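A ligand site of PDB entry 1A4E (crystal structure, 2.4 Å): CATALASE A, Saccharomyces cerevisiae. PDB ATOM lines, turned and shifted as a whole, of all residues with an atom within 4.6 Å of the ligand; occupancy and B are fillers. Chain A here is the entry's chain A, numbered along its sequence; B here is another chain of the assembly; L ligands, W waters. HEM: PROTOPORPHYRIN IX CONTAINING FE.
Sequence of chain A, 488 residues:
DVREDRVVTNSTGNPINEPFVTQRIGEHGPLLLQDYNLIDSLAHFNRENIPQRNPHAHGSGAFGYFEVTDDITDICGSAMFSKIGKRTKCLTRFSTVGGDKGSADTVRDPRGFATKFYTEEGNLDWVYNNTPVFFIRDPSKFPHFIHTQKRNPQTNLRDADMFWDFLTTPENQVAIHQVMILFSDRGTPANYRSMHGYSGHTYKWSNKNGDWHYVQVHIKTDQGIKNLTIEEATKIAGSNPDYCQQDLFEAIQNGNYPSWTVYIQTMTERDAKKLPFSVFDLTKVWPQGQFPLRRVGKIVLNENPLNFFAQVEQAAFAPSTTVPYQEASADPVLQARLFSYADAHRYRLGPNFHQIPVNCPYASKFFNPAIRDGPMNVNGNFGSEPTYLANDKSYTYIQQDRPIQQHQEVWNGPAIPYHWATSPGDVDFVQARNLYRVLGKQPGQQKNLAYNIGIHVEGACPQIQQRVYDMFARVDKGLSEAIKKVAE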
ATOM      1  N   ARG A  53      23.619  33.186 -17.783  1.00  0.00           N
ATOM      2  CA  ARG A  53      24.080  31.826 -17.488  1.00  0.00           C
ATOM      3  C   ARG A  53      23.266  31.193 -16.375  1.00  0.00           C
ATOM      4  O   ARG A  53      22.801  31.864 -15.447  1.00  0.00           O
ATOM      5  CB  ARG A  53      25.535  31.832 -17.054  1.00  0.00           C
ATOM      6  CG  ARG A  53      26.518  32.250 -18.118  1.00  0.00           C
ATOM      7  CD  ARG A  53      27.845  32.594 -17.464  1.00  0.00           C
ATOM      8  NE  ARG A  53      28.441  33.748 -18.119  1.00  0.00           N
ATOM      9  CZ  ARG A  53      29.278  33.628 -19.149  1.00  0.00           C
ATOM     10  NH1 ARG A  53      29.600  32.428 -19.639  1.00  0.00           N
ATOM     11  NH2 ARG A  53      29.832  34.687 -19.685  1.00  0.00           N
ATOM     12  N   ASN A  54      23.089  29.879 -16.484  1.00  0.00           N
ATOM     13  CA  ASN A  54      22.381  29.139 -15.467  1.00  0.00           C
ATOM     14  C   ASN A  54      23.265  27.971 -15.037  1.00  0.00           C
ATOM     15  O   ASN A  54      23.452  27.019 -15.793  1.00  0.00           O
ATOM     16  CB  ASN A  54      21.056  28.683 -16.069  1.00  0.00           C
ATOM     17  CG  ASN A  54      20.054  28.206 -15.044  1.00  0.00           C
ATOM     18  OD1 ASN A  54      20.071  28.600 -13.882  1.00  0.00           O
ATOM     19  ND2 ASN A  54      19.150  27.319 -15.459  1.00  0.00           N
ATOM     20  N   PRO A  55      23.928  28.010 -13.863  1.00  0.00           N
ATOM     21  CA  PRO A  55      23.986  29.131 -12.939  1.00  0.00           C
ATOM     22  C   PRO A  55      25.178  30.019 -13.251  1.00  0.00           C
ATOM     23  O   PRO A  55      25.657  30.030 -14.387  1.00  0.00           O
ATOM     24  CB  PRO A  55      24.061  28.454 -11.587  1.00  0.00           C
ATOM     25  CG  PRO A  55      24.290  26.981 -11.858  1.00  0.00           C
ATOM     26  CD  PRO A  55      24.708  26.918 -13.309  1.00  0.00           C
ATOM     27  N   HIS A  56      25.712  30.753 -12.259  1.00  0.00           N
ATOM     28  CA  HIS A  56      26.853  31.654 -12.408  1.00  0.00           C
ATOM     29  C   HIS A  56      26.596  32.826 -13.340  1.00  0.00           C
ATOM     30  O   HIS A  56      27.453  33.281 -14.100  1.00  0.00           O
ATOM     31  CB  HIS A  56      28.088  30.890 -12.913  1.00  0.00           C
ATOM     32  CG  HIS A  56      28.688  29.882 -11.942  1.00  0.00           C
ATOM     33  ND1 HIS A  56      29.819  30.021 -11.262  1.00  0.00           N
ATOM     34  CD2 HIS A  56      28.171  28.633 -11.660  1.00  0.00           C
ATOM     35  CE1 HIS A  56      30.030  28.915 -10.591  1.00  0.00           C
ATOM     36  NE2 HIS A  56      29.038  28.099 -10.833  1.00  0.00           N
ATOM     37  N   ARG A  93      37.154  34.066 -16.048  1.00  0.00           N
ATOM     38  CA  ARG A  93      35.935  34.688 -15.577  1.00  0.00           C
ATOM     39  C   ARG A  93      35.673  34.135 -14.183  1.00  0.00           C
ATOM     40  O   ARG A  93      35.643  32.924 -13.954  1.00  0.00           O
ATOM     41  CB  ARG A  93      34.748  34.370 -16.478  1.00  0.00           C
ATOM     42  CG  ARG A  93      33.472  35.113 -16.078  1.00  0.00           C
ATOM     43  CD  ARG A  93      32.360  34.764 -17.046  1.00  0.00           C
ATOM     44  NE  ARG A  93      31.124  35.462 -16.785  1.00  0.00           N
ATOM     45  CZ  ARG A  93      30.194  35.057 -15.897  1.00  0.00           C
ATOM     46  NH1 ARG A  93      30.367  33.951 -15.174  1.00  0.00           N
ATOM     47  NH2 ARG A  93      29.041  35.698 -15.770  1.00  0.00           N
ATOM     48  N   SER A  95      32.989  34.401 -10.791  1.00  0.00           N
ATOM     49  CA  SER A  95      31.563  34.577 -10.672  1.00  0.00           C
ATOM     50  C   SER A  95      31.001  34.064  -9.350  1.00  0.00           C
ATOM     51  O   SER A  95      31.709  33.420  -8.577  1.00  0.00           O
ATOM     52  CB  SER A  95      30.850  33.838 -11.807  1.00  0.00           C
ATOM     53  OG  SER A  95      31.136  32.450 -11.829  1.00  0.00           O
ATOM     54  N   GLY A 112      32.983  30.920  -8.943  1.00  0.00           N
ATOM     55  CA  GLY A 112      33.566  30.250 -10.088  1.00  0.00           C
ATOM     56  C   GLY A 112      34.923  30.868 -10.418  1.00  0.00           C
ATOM     57  O   GLY A 112      35.208  32.032 -10.132  1.00  0.00           O
ATOM     58  N   PHE A 113      35.768  30.052 -11.040  1.00  0.00           N
ATOM     59  CA  PHE A 113      37.115  30.434 -11.439  1.00  0.00           C
ATOM     60  C   PHE A 113      37.352  29.595 -12.688  1.00  0.00           C
ATOM     61  O   PHE A 113      37.912  28.494 -12.650  1.00  0.00           O
ATOM     62  CB  PHE A 113      38.106  30.066 -10.313  1.00  0.00           C
ATOM     63  CG  PHE A 113      39.536  30.611 -10.426  1.00  0.00           C
ATOM     64  CD1 PHE A 113      40.146  30.915 -11.644  1.00  0.00           C
ATOM     65  CD2 PHE A 113      40.271  30.799  -9.243  1.00  0.00           C
ATOM     66  CE1 PHE A 113      41.451  31.389 -11.689  1.00  0.00           C
ATOM     67  CE2 PHE A 113      41.576  31.272  -9.288  1.00  0.00           C
ATOM     68  CZ  PHE A 113      42.166  31.581 -10.514  1.00  0.00           C
ATOM     69  N   ALA A 114      36.867  30.150 -13.800  1.00  0.00           N
ATOM     70  CA  ALA A 114      36.953  29.498 -15.098  1.00  0.00           C
ATOM     71  C   ALA A 114      38.038  30.100 -15.969  1.00  0.00           C
ATOM     72  O   ALA A 114      38.027  31.307 -16.211  1.00  0.00           O
ATOM     73  CB  ALA A 114      35.600  29.629 -15.788  1.00  0.00           C
ATOM     74  N   VAL A 127      37.333  24.777 -15.935  1.00  0.00           N
ATOM     75  CA  VAL A 127      36.116  25.307 -15.342  1.00  0.00           C
ATOM     76  C   VAL A 127      36.050  24.844 -13.890  1.00  0.00           C
ATOM     77  O   VAL A 127      35.516  23.787 -13.540  1.00  0.00           O
ATOM     78  CB  VAL A 127      34.894  24.810 -16.149  1.00  0.00           C
ATOM     79  CG1 VAL A 127      33.665  25.590 -15.719  1.00  0.00           C
ATOM     80  CG2 VAL A 127      35.106  25.020 -17.638  1.00  0.00           C
ATOM     81  N   TYR A 128      36.649  25.684 -13.043  1.00  0.00           N
ATOM     82  CA  TYR A 128      36.844  25.373 -11.640  1.00  0.00           C
ATOM     83  C   TYR A 128      36.010  26.225 -10.702  1.00  0.00           C
ATOM     84  O   TYR A 128      35.534  27.278 -11.098  1.00  0.00           O
ATOM     85  CB  TYR A 128      38.308  25.562 -11.266  1.00  0.00           C
ATOM     86  CG  TYR A 128      39.338  24.646 -11.928  1.00  0.00           C
ATOM     87  CD1 TYR A 128      38.975  23.622 -12.806  1.00  0.00           C
ATOM     88  CD2 TYR A 128      40.681  24.823 -11.591  1.00  0.00           C
ATOM     89  CE1 TYR A 128      39.944  22.773 -13.361  1.00  0.00           C
ATOM     90  CE2 TYR A 128      41.667  23.985 -12.132  1.00  0.00           C
ATOM     91  CZ  TYR A 128      41.280  22.968 -13.008  1.00  0.00           C
ATOM     92  OH  TYR A 128      42.236  22.140 -13.528  1.00  0.00           O
ATOM     93  N   ASN A 129      35.813  25.777  -9.454  1.00  0.00           N
ATOM     94  CA  ASN A 129      35.238  26.594  -8.406  1.00  0.00           C
ATOM     95  C   ASN A 129      36.300  26.915  -7.386  1.00  0.00           C
ATOM     96  O   ASN A 129      37.397  26.352  -7.427  1.00  0.00           O
ATOM     97  CB  ASN A 129      34.103  25.895  -7.703  1.00  0.00           C
ATOM     98  CG  ASN A 129      32.787  26.078  -8.434  1.00  0.00           C
ATOM     99  OD1 ASN A 129      32.584  27.040  -9.185  1.00  0.00           O
ATOM    100  ND2 ASN A 129      31.856  25.151  -8.234  1.00  0.00           N
ATOM    101  N   PHE A 134      32.300  19.743  -3.954  1.00  0.00           N
ATOM    102  CA  PHE A 134      31.003  20.305  -4.306  1.00  0.00           C
ATOM    103  C   PHE A 134      29.897  19.539  -3.583  1.00  0.00           C
ATOM    104  O   PHE A 134      30.108  18.515  -2.936  1.00  0.00           O
ATOM    105  CB  PHE A 134      30.819  20.236  -5.822  1.00  0.00           C
ATOM    106  CG  PHE A 134      29.823  21.226  -6.417  1.00  0.00           C
ATOM    107  CD1 PHE A 134      30.014  22.602  -6.250  1.00  0.00           C
ATOM    108  CD2 PHE A 134      28.712  20.744  -7.128  1.00  0.00           C
ATOM    109  CE1 PHE A 134      29.106  23.500  -6.812  1.00  0.00           C
ATOM    110  CE2 PHE A 134      27.811  21.650  -7.689  1.00  0.00           C
ATOM    111  CZ  PHE A 134      28.011  23.018  -7.528  1.00  0.00           C
ATOM    112  N   ILE A 136      27.261  17.838  -4.660  1.00  0.00           N
ATOM    113  CA  ILE A 136      26.658  16.613  -5.176  1.00  0.00           C
ATOM    114  C   ILE A 136      27.656  15.669  -5.822  1.00  0.00           C
ATOM    115  O   ILE A 136      28.728  16.092  -6.253  1.00  0.00           O
ATOM    116  CB  ILE A 136      25.532  16.931  -6.230  1.00  0.00           C
ATOM    117  CG1 ILE A 136      26.091  17.810  -7.361  1.00  0.00           C
ATOM    118  CG2 ILE A 136      24.342  17.612  -5.558  1.00  0.00           C
ATOM    119  CD1 ILE A 136      25.168  17.801  -8.592  1.00  0.00           C
ATOM    120  N   PRO A 139      24.809  13.574 -10.932  1.00  0.00           N
ATOM    121  CA  PRO A 139      24.551  14.646 -11.901  1.00  0.00           C
ATOM    122  C   PRO A 139      23.085  15.051 -12.014  1.00  0.00           C
ATOM    123  O   PRO A 139      22.759  16.227 -12.160  1.00  0.00           O
ATOM    124  CB  PRO A 139      25.145  14.098 -13.170  1.00  0.00           C
ATOM    125  CG  PRO A 139      24.984  12.600 -13.029  1.00  0.00           C
ATOM    126  CD  PRO A 139      25.368  12.399 -11.574  1.00  0.00           C
ATOM    127  N   PHE A 142      21.694  17.995  -9.868  1.00  0.00           N
ATOM    128  CA  PHE A 142      22.037  19.391 -10.134  1.00  0.00           C
ATOM    129  C   PHE A 142      20.893  20.346 -10.452  1.00  0.00           C
ATOM    130  O   PHE A 142      20.901  21.410  -9.833  1.00  0.00           O
ATOM    131  CB  PHE A 142      23.054  19.472 -11.280  1.00  0.00           C
ATOM    132  CG  PHE A 142      23.657  20.852 -11.492  1.00  0.00           C
ATOM    133  CD1 PHE A 142      24.635  21.324 -10.610  1.00  0.00           C
ATOM    134  CD2 PHE A 142      23.245  21.644 -12.579  1.00  0.00           C
ATOM    135  CE1 PHE A 142      25.208  22.582 -10.811  1.00  0.00           C
ATOM    136  CE2 PHE A 142      23.823  22.898 -12.767  1.00  0.00           C
ATOM    137  CZ  PHE A 142      24.811  23.362 -11.891  1.00  0.00           C
ATOM    138  N   SER A 199      40.249  22.050  -9.245  1.00  0.00           N
ATOM    139  CA  SER A 199      39.548  21.246 -10.227  1.00  0.00           C
ATOM    140  C   SER A 199      38.317  20.563  -9.654  1.00  0.00           C
ATOM    141  O   SER A 199      37.319  20.393 -10.371  1.00  0.00           O
ATOM    142  CB  SER A 199      40.492  20.173 -10.826  1.00  0.00           C
ATOM    143  OG  SER A 199      40.943  19.168  -9.924  1.00  0.00           O
ATOM    144  N   HIS A 201      37.072  17.798  -9.368  1.00  0.00           N
ATOM    145  CA  HIS A 201      37.132  16.471  -9.909  1.00  0.00           C
ATOM    146  C   HIS A 201      38.562  16.025 -10.130  1.00  0.00           C
ATOM    147  O   HIS A 201      39.511  16.810 -10.246  1.00  0.00           O
ATOM    148  CB  HIS A 201      36.447  16.391 -11.265  1.00  0.00           C
ATOM    149  CG  HIS A 201      35.070  17.007 -11.344  1.00  0.00           C
ATOM    150  ND1 HIS A 201      33.935  16.601 -10.808  1.00  0.00           N
ATOM    151  CD2 HIS A 201      34.792  18.125 -12.092  1.00  0.00           C
ATOM    152  CE1 HIS A 201      32.987  17.409 -11.187  1.00  0.00           C
ATOM    153  NE2 HIS A 201      33.515  18.330 -11.962  1.00  0.00           N
ATOM    154  N   LEU A 282      33.449  13.566  -5.988  1.00  0.00           N
ATOM    155  CA  LEU A 282      33.623  15.021  -5.936  1.00  0.00           C
ATOM    156  C   LEU A 282      33.598  15.582  -4.518  1.00  0.00           C
ATOM    157  O   LEU A 282      34.200  16.613  -4.278  1.00  0.00           O
ATOM    158  CB  LEU A 282      32.514  15.728  -6.678  1.00  0.00           C
ATOM    159  CG  LEU A 282      32.750  16.937  -7.586  1.00  0.00           C
ATOM    160  CD1 LEU A 282      31.375  17.513  -7.806  1.00  0.00           C
ATOM    161  CD2 LEU A 282      33.665  17.997  -7.016  1.00  0.00           C
ATOM    162  N   PHE A 317      32.749  28.777 -21.537  1.00  0.00           N
ATOM    163  CA  PHE A 317      33.671  27.833 -20.910  1.00  0.00           C
ATOM    164  C   PHE A 317      32.995  26.483 -20.758  1.00  0.00           C
ATOM    165  O   PHE A 317      31.839  26.399 -20.348  1.00  0.00           O
ATOM    166  CB  PHE A 317      34.102  28.299 -19.521  1.00  0.00           C
ATOM    167  CG  PHE A 317      34.789  29.647 -19.488  1.00  0.00           C
ATOM    168  CD1 PHE A 317      34.013  30.811 -19.372  1.00  0.00           C
ATOM    169  CD2 PHE A 317      36.175  29.738 -19.559  1.00  0.00           C
ATOM    170  CE1 PHE A 317      34.640  32.052 -19.330  1.00  0.00           C
ATOM    171  CE2 PHE A 317      36.799  30.994 -19.510  1.00  0.00           C
ATOM    172  CZ  PHE A 317      36.026  32.142 -19.401  1.00  0.00           C
ATOM    173  N   VAL A 333      29.603  13.502 -12.052  1.00  0.00           N
ATOM    174  CA  VAL A 333      29.294  14.913 -12.180  1.00  0.00           C
ATOM    175  C   VAL A 333      30.112  15.495 -13.336  1.00  0.00           C
ATOM    176  O   VAL A 333      29.517  16.143 -14.191  1.00  0.00           O
ATOM    177  CB  VAL A 333      29.599  15.623 -10.841  1.00  0.00           C
ATOM    178  CG1 VAL A 333      29.396  17.121 -10.907  1.00  0.00           C
ATOM    179  CG2 VAL A 333      28.646  15.064  -9.807  1.00  0.00           C
ATOM    180  N   ALA A 336      28.697  14.314 -16.780  1.00  0.00           N
ATOM    181  CA  ALA A 336      27.541  15.095 -17.221  1.00  0.00           C
ATOM    182  C   ALA A 336      27.906  16.506 -17.686  1.00  0.00           C
ATOM    183  O   ALA A 336      27.308  17.046 -18.619  1.00  0.00           O
ATOM    184  CB  ALA A 336      26.535  15.245 -16.112  1.00  0.00           C
ATOM    185  N   ARG A 337      28.931  17.095 -17.042  1.00  0.00           N
ATOM    186  CA  ARG A 337      29.430  18.407 -17.404  1.00  0.00           C
ATOM    187  C   ARG A 337      30.066  18.416 -18.787  1.00  0.00           C
ATOM    188  O   ARG A 337      30.135  19.476 -19.414  1.00  0.00           O
ATOM    189  CB  ARG A 337      30.459  18.889 -16.401  1.00  0.00           C
ATOM    190  CG  ARG A 337      29.864  19.162 -15.021  1.00  0.00           C
ATOM    191  CD  ARG A 337      30.925  19.593 -14.031  1.00  0.00           C
ATOM    192  NE  ARG A 337      31.330  20.971 -14.253  1.00  0.00           N
ATOM    193  CZ  ARG A 337      32.589  21.396 -14.081  1.00  0.00           C
ATOM    194  NH1 ARG A 337      33.574  20.582 -13.701  1.00  0.00           N
ATOM    195  NH2 ARG A 337      32.878  22.672 -14.281  1.00  0.00           N
ATOM    196  N   SER A 340      26.731  19.266 -20.673  1.00  0.00           N
ATOM    197  CA  SER A 340      25.973  20.458 -20.332  1.00  0.00           C
ATOM    198  C   SER A 340      26.406  21.822 -20.788  1.00  0.00           C
ATOM    199  O   SER A 340      25.560  22.616 -21.227  1.00  0.00           O
ATOM    200  CB  SER A 340      25.806  20.538 -18.836  1.00  0.00           C
ATOM    201  OG  SER A 340      24.992  19.473 -18.393  1.00  0.00           O
ATOM    202  N   TYR A 341      27.701  22.111 -20.741  1.00  0.00           N
ATOM    203  CA  TYR A 341      28.152  23.467 -21.009  1.00  0.00           C
ATOM    204  C   TYR A 341      28.077  23.814 -22.476  1.00  0.00           C
ATOM    205  O   TYR A 341      27.498  24.842 -22.795  1.00  0.00           O
ATOM    206  CB  TYR A 341      29.565  23.659 -20.493  1.00  0.00           C
ATOM    207  CG  TYR A 341      29.706  23.633 -18.975  1.00  0.00           C
ATOM    208  CD1 TYR A 341      29.350  22.503 -18.236  1.00  0.00           C
ATOM    209  CD2 TYR A 341      30.194  24.758 -18.319  1.00  0.00           C
ATOM    210  CE1 TYR A 341      29.485  22.482 -16.848  1.00  0.00           C
ATOM    211  CE2 TYR A 341      30.336  24.744 -16.930  1.00  0.00           C
ATOM    212  CZ  TYR A 341      29.980  23.603 -16.211  1.00  0.00           C
ATOM    213  OH  TYR A 341      30.054  23.608 -14.826  1.00  0.00           O
ATOM    214  N   ALA A 344      24.611  24.413 -23.393  1.00  0.00           N
ATOM    215  CA  ALA A 344      24.152  25.705 -22.920  1.00  0.00           C
ATOM    216  C   ALA A 344      24.650  26.835 -23.805  1.00  0.00           C
ATOM    217  O   ALA A 344      23.926  27.793 -24.041  1.00  0.00           O
ATOM    218  CB  ALA A 344      24.645  25.956 -21.496  1.00  0.00           C
ATOM    219  N   HIS A 345      25.863  26.715 -24.363  1.00  0.00           N
ATOM    220  CA  HIS A 345      26.411  27.734 -25.234  1.00  0.00           C
ATOM    221  C   HIS A 345      25.649  27.809 -26.555  1.00  0.00           C
ATOM    222  O   HIS A 345      25.503  28.887 -27.116  1.00  0.00           O
ATOM    223  CB  HIS A 345      27.876  27.453 -25.546  1.00  0.00           C
ATOM    224  CG  HIS A 345      28.766  27.307 -24.330  1.00  0.00           C
ATOM    225  ND1 HIS A 345      29.864  26.573 -24.247  1.00  0.00           N
ATOM    226  CD2 HIS A 345      28.573  27.899 -23.100  1.00  0.00           C
ATOM    227  CE1 HIS A 345      30.345  26.683 -23.036  1.00  0.00           C
ATOM    228  NE2 HIS A 345      29.563  27.477 -22.348  1.00  0.00           N
ATOM    229  N   ARG A 348      22.273  29.816 -25.257  1.00  0.00           N
ATOM    230  CA  ARG A 348      22.603  31.144 -24.751  1.00  0.00           C
ATOM    231  C   ARG A 348      23.279  32.067 -25.745  1.00  0.00           C
ATOM    232  O   ARG A 348      22.934  33.243 -25.854  1.00  0.00           O
ATOM    233  CB  ARG A 348      23.484  30.964 -23.522  1.00  0.00           C
ATOM    234  CG  ARG A 348      23.842  32.231 -22.773  1.00  0.00           C
ATOM    235  CD  ARG A 348      24.574  31.946 -21.457  1.00  0.00           C
ATOM    236  NE  ARG A 348      25.904  31.380 -21.604  1.00  0.00           N
ATOM    237  CZ  ARG A 348      26.991  32.109 -21.816  1.00  0.00           C
ATOM    238  NH1 ARG A 348      26.936  33.427 -21.995  1.00  0.00           N
ATOM    239  NH2 ARG A 348      28.173  31.508 -21.929  1.00  0.00           N
ATOM    240  N   LEU B  42      18.867  17.910 -18.028  1.00  0.00           N
ATOM    241  CA  LEU B  42      19.962  18.871 -18.117  1.00  0.00           C
ATOM    242  C   LEU B  42      19.789  19.873 -19.248  1.00  0.00           C
ATOM    243  O   LEU B  42      20.087  21.052 -19.078  1.00  0.00           O
ATOM    244  CB  LEU B  42      21.291  18.123 -18.276  1.00  0.00           C
ATOM    245  CG  LEU B  42      21.797  17.304 -17.080  1.00  0.00           C
ATOM    246  CD1 LEU B  42      23.127  16.693 -17.432  1.00  0.00           C
ATOM    247  CD2 LEU B  42      21.942  18.175 -15.852  1.00  0.00           C
ATOM    248  N   ASN B  46      19.303  23.985 -19.043  1.00  0.00           N
ATOM    249  CA  ASN B  46      20.053  24.966 -19.811  1.00  0.00           C
ATOM    250  C   ASN B  46      19.230  26.008 -20.550  1.00  0.00           C
ATOM    251  O   ASN B  46      19.765  27.034 -20.990  1.00  0.00           O
ATOM    252  CB  ASN B  46      20.932  24.268 -20.824  1.00  0.00           C
ATOM    253  CG  ASN B  46      22.072  23.496 -20.209  1.00  0.00           C
ATOM    254  OD1 ASN B  46      22.397  23.665 -19.038  1.00  0.00           O
ATOM    255  ND2 ASN B  46      22.718  22.643 -20.995  1.00  0.00           N
HETATM  256  CHA HEM L   1      28.615  27.264 -15.104  1.00  0.00           C
HETATM  257  CHB HEM L   1      26.315  23.078 -15.446  1.00  0.00           C
HETATM  258  CHC HEM L   1      28.923  21.384 -11.766  1.00  0.00           C
HETATM  259  CHD HEM L   1      31.809  25.185 -12.159  1.00  0.00           C
HETATM  260  C1A HEM L   1      27.673  26.321 -15.426  1.00  0.00           C
HETATM  261  C2A HEM L   1      26.742  26.451 -16.524  1.00  0.00           C
HETATM  262  C3A HEM L   1      26.133  25.244 -16.662  1.00  0.00           C
HETATM  263  C4A HEM L   1      26.683  24.393 -15.648  1.00  0.00           C
HETATM  264  CMA HEM L   1      25.132  24.837 -17.733  1.00  0.00           C
HETATM  265  CAA HEM L   1      26.549  27.655 -17.408  1.00  0.00           C
HETATM  266  CBA HEM L   1      27.372  27.560 -18.692  1.00  0.00           C
HETATM  267  CGA HEM L   1      27.065  28.640 -19.720  1.00  0.00           C
HETATM  268  O1A HEM L   1      25.905  28.941 -19.953  1.00  0.00           O
HETATM  269  O2A HEM L   1      28.002  29.179 -20.310  1.00  0.00           O
HETATM  270  C1B HEM L   1      26.843  22.225 -14.481  1.00  0.00           C
HETATM  271  C2B HEM L   1      26.341  20.900 -14.225  1.00  0.00           C
HETATM  272  C3B HEM L   1      27.000  20.447 -13.106  1.00  0.00           C
HETATM  273  C4B HEM L   1      27.939  21.506 -12.741  1.00  0.00           C
HETATM  274  CMB HEM L   1      25.294  20.207 -15.081  1.00  0.00           C
HETATM  275  CAB HEM L   1      26.844  19.254 -12.399  1.00  0.00           C
HETATM  276  CBB HEM L   1      26.377  17.978 -12.905  1.00  0.00           C
HETATM  277  C1C HEM L   1      29.949  22.279 -11.536  1.00  0.00           C
HETATM  278  C2C HEM L   1      31.114  21.980 -10.739  1.00  0.00           C
HETATM  279  C3C HEM L   1      31.999  22.999 -10.938  1.00  0.00           C
HETATM  280  C4C HEM L   1      31.324  23.942 -11.815  1.00  0.00           C
HETATM  281  CMC HEM L   1      31.294  20.736  -9.873  1.00  0.00           C
HETATM  282  CAC HEM L   1      33.301  23.133 -10.479  1.00  0.00           C
HETATM  283  CBC HEM L   1      34.342  22.119 -10.536  1.00  0.00           C
HETATM  284  C1D HEM L   1      31.162  26.098 -12.970  1.00  0.00           C
HETATM  285  C2D HEM L   1      31.679  27.404 -13.293  1.00  0.00           C
HETATM  286  C3D HEM L   1      30.767  27.989 -14.111  1.00  0.00           C
HETATM  287  C4D HEM L   1      29.689  27.054 -14.277  1.00  0.00           C
HETATM  288  CMD HEM L   1      33.014  27.985 -12.836  1.00  0.00           C
HETATM  289  CAD HEM L   1      30.824  29.375 -14.724  1.00  0.00           C
HETATM  290  CBD HEM L   1      31.631  29.490 -15.995  1.00  0.00           C
HETATM  291  CGD HEM L   1      31.603  30.923 -16.494  1.00  0.00           C
HETATM  292  O1D HEM L   1      32.196  31.789 -15.856  1.00  0.00           O
HETATM  293  O2D HEM L   1      30.991  31.194 -17.514  1.00  0.00           O
HETATM  294  NA  HEM L   1      27.657  25.041 -14.904  1.00  0.00           N
HETATM  295  NB  HEM L   1      27.825  22.600 -13.581  1.00  0.00           N
HETATM  296  NC  HEM L   1      30.088  23.469 -12.216  1.00  0.00           N
HETATM  297  ND  HEM L   1      29.943  25.882 -13.580  1.00  0.00           N
HETATM  298 FE   HEM L   1      28.856  24.273 -13.536  1.00  0.00          FE
HETATM  299  O   HOH W   1      33.338  31.641 -13.251  1.00  0.00           O
HETATM  300  O   HOH W   2      36.514  21.096 -12.962  1.00  0.00           O
HETATM  301  O   HOH W   3      22.363  26.393 -18.238  1.00  0.00           O
HETATM  302  O   HOH W   4      23.198  28.830 -19.366  1.00  0.00           O
HETATM  303  O   HOH W   5      30.647  29.414 -19.660  1.00  0.00           O
HETATM  304  O   HOH W   6      36.093  22.996  -7.687  1.00  0.00           O
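FE of the ligand is bound by OH of Tyr 341 (1.9 Å). NH1 of Arg 93 is in salt-bridge range of O1D of the ligand, 2.9 Å away. An oxygen (O2A) of the ligand is in salt-bridge range of the guanidinium group (NH2) of Arg 348, 2.8 Å away. O2D of the ligand lies within salt-bridge range of NH1 of Arg 53 (2.8 Å). A ring nitrogen (NE2) of His 345 lies within hydrogen-bond range of an oxygen (O2A) of the ligand (3.1 Å).
The guanidinium group of Arg 337 sits close to a nitrogen (NC) of the ligand (3.5 Å). Asn 54 touches the ligand. Pro 55 touches the ligand. His 56 touches the ligand. Gly 112 touches the ligand. Phe 113 touches the ligand. CB of Ala 114 touches CBD of the ligand, at 3.98 Å. CG1 of Val 127 touches C2D of the ligand, 3.6 Å away. Tyr 128 touches the ligand (O to CMD, 3.1 Å). ND2 of Asn 129 touches CAC of the ligand (3.3 Å). CD2 of Phe 134 touches CMC of the ligand, 3.8 Å away. CA of Pro 139 touches CBB of the ligand (3.9 Å). Phe 142 touches the ligand. Ser 199 touches the ligand (O to CBC, 3.4 Å). His 201 touches the ligand (NE2 to CMC, 3.9 Å). CD1 of Leu 282 touches CMC of the ligand, at 3.8 Å. Phe 317 touches the ligand (CD1 to O2D, 3.6 Å). CG1 of Val 333 touches CAB of the ligand, 3.6 Å away. Ser 340 touches the ligand. CB of Ala 344 touches O1A of the ligand (3.6 Å). Leu 42 of chain B touches the ligand (CD2 to CMB, 3.99 Å). OD1 of Asn 46 of chain B touches CMA of the ligand (3.2 Å). Hydrophobic or aromatic side chains within 4 Å of the ligand: Pro 55, His 56, Ala 114, Val 127, Phe 134, Phe 142, His 201, Leu 282, Phe 317, Val 333, Tyr 341, Ala 344, His 345 and Leu 42 of chain B.
Water W5 lies within hydrogen-bond range of an oxygen (O2A) of the ligand (2.7 Å), the backbone NH of Phe 317 (2.9 Å), the guanidinium group of Arg 53 (3.2 Å) and a ring nitrogen (NE2) of His 345 (3.5 Å). Water W4 lies within hydrogen-bond range of an oxygen (O1A) of the ligand (2.8 Å) and the backbone NH of Asn 54 (3.1 Å). Water W1 lies within hydrogen-bond range of O of Arg 93, OG of Ser 95 and O1D of the ligand. Water W3 bridges the backbone carbonyl oxygen (O) of Asn 54 and the side-chain amide oxygen (OD1) of Asn 46 of chain B. Water W2 lies within hydrogen-bond range of the backbone carbonyl oxygen of Ser 199 (2.8 Å), the backbone carbonyl oxygen of Val 127 (2.9 Å) and the guanidinium group of Arg 337 (3.1 Å).
The guanidinium group (NE) of Arg 337 sits close to the side-chain hydroxyl (OH) of Tyr 341 (3.0 Å). The guanidinium group (NH1) of Arg 337 is in hydrogen-bond range of a ring nitrogen (NE2) of His 201 (2.8 Å). The backbone carbonyl oxygen of Ser 340 sits at hydrogen-bond distance from the side-chain amide nitrogen of Asn 46 of chain B (2.9 Å). The backbone carbonyl oxygen of Tyr 341 lies close to a ring nitrogen (ND1) of His 345 (3.3 Å). The backbone carbonyl oxygen of Ser 95 sits at hydrogen-bond distance from the backbone NH of Gly 112 (2.8 Å). A ring nitrogen (NE2) of His 345 sits close to the backbone carbonyl oxygen (O) of Phe 317, at 3.2 Å. The side-chain hydroxyl of Ser 199 lies within hydrogen-bond range of the backbone carbonyl oxygen of His 201, 2.8 Å away. A ring nitrogen (ND1) of His 56 lies within hydrogen-bond range of the side-chain hydroxyl (OG) of Ser 95 (2.8 Å).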
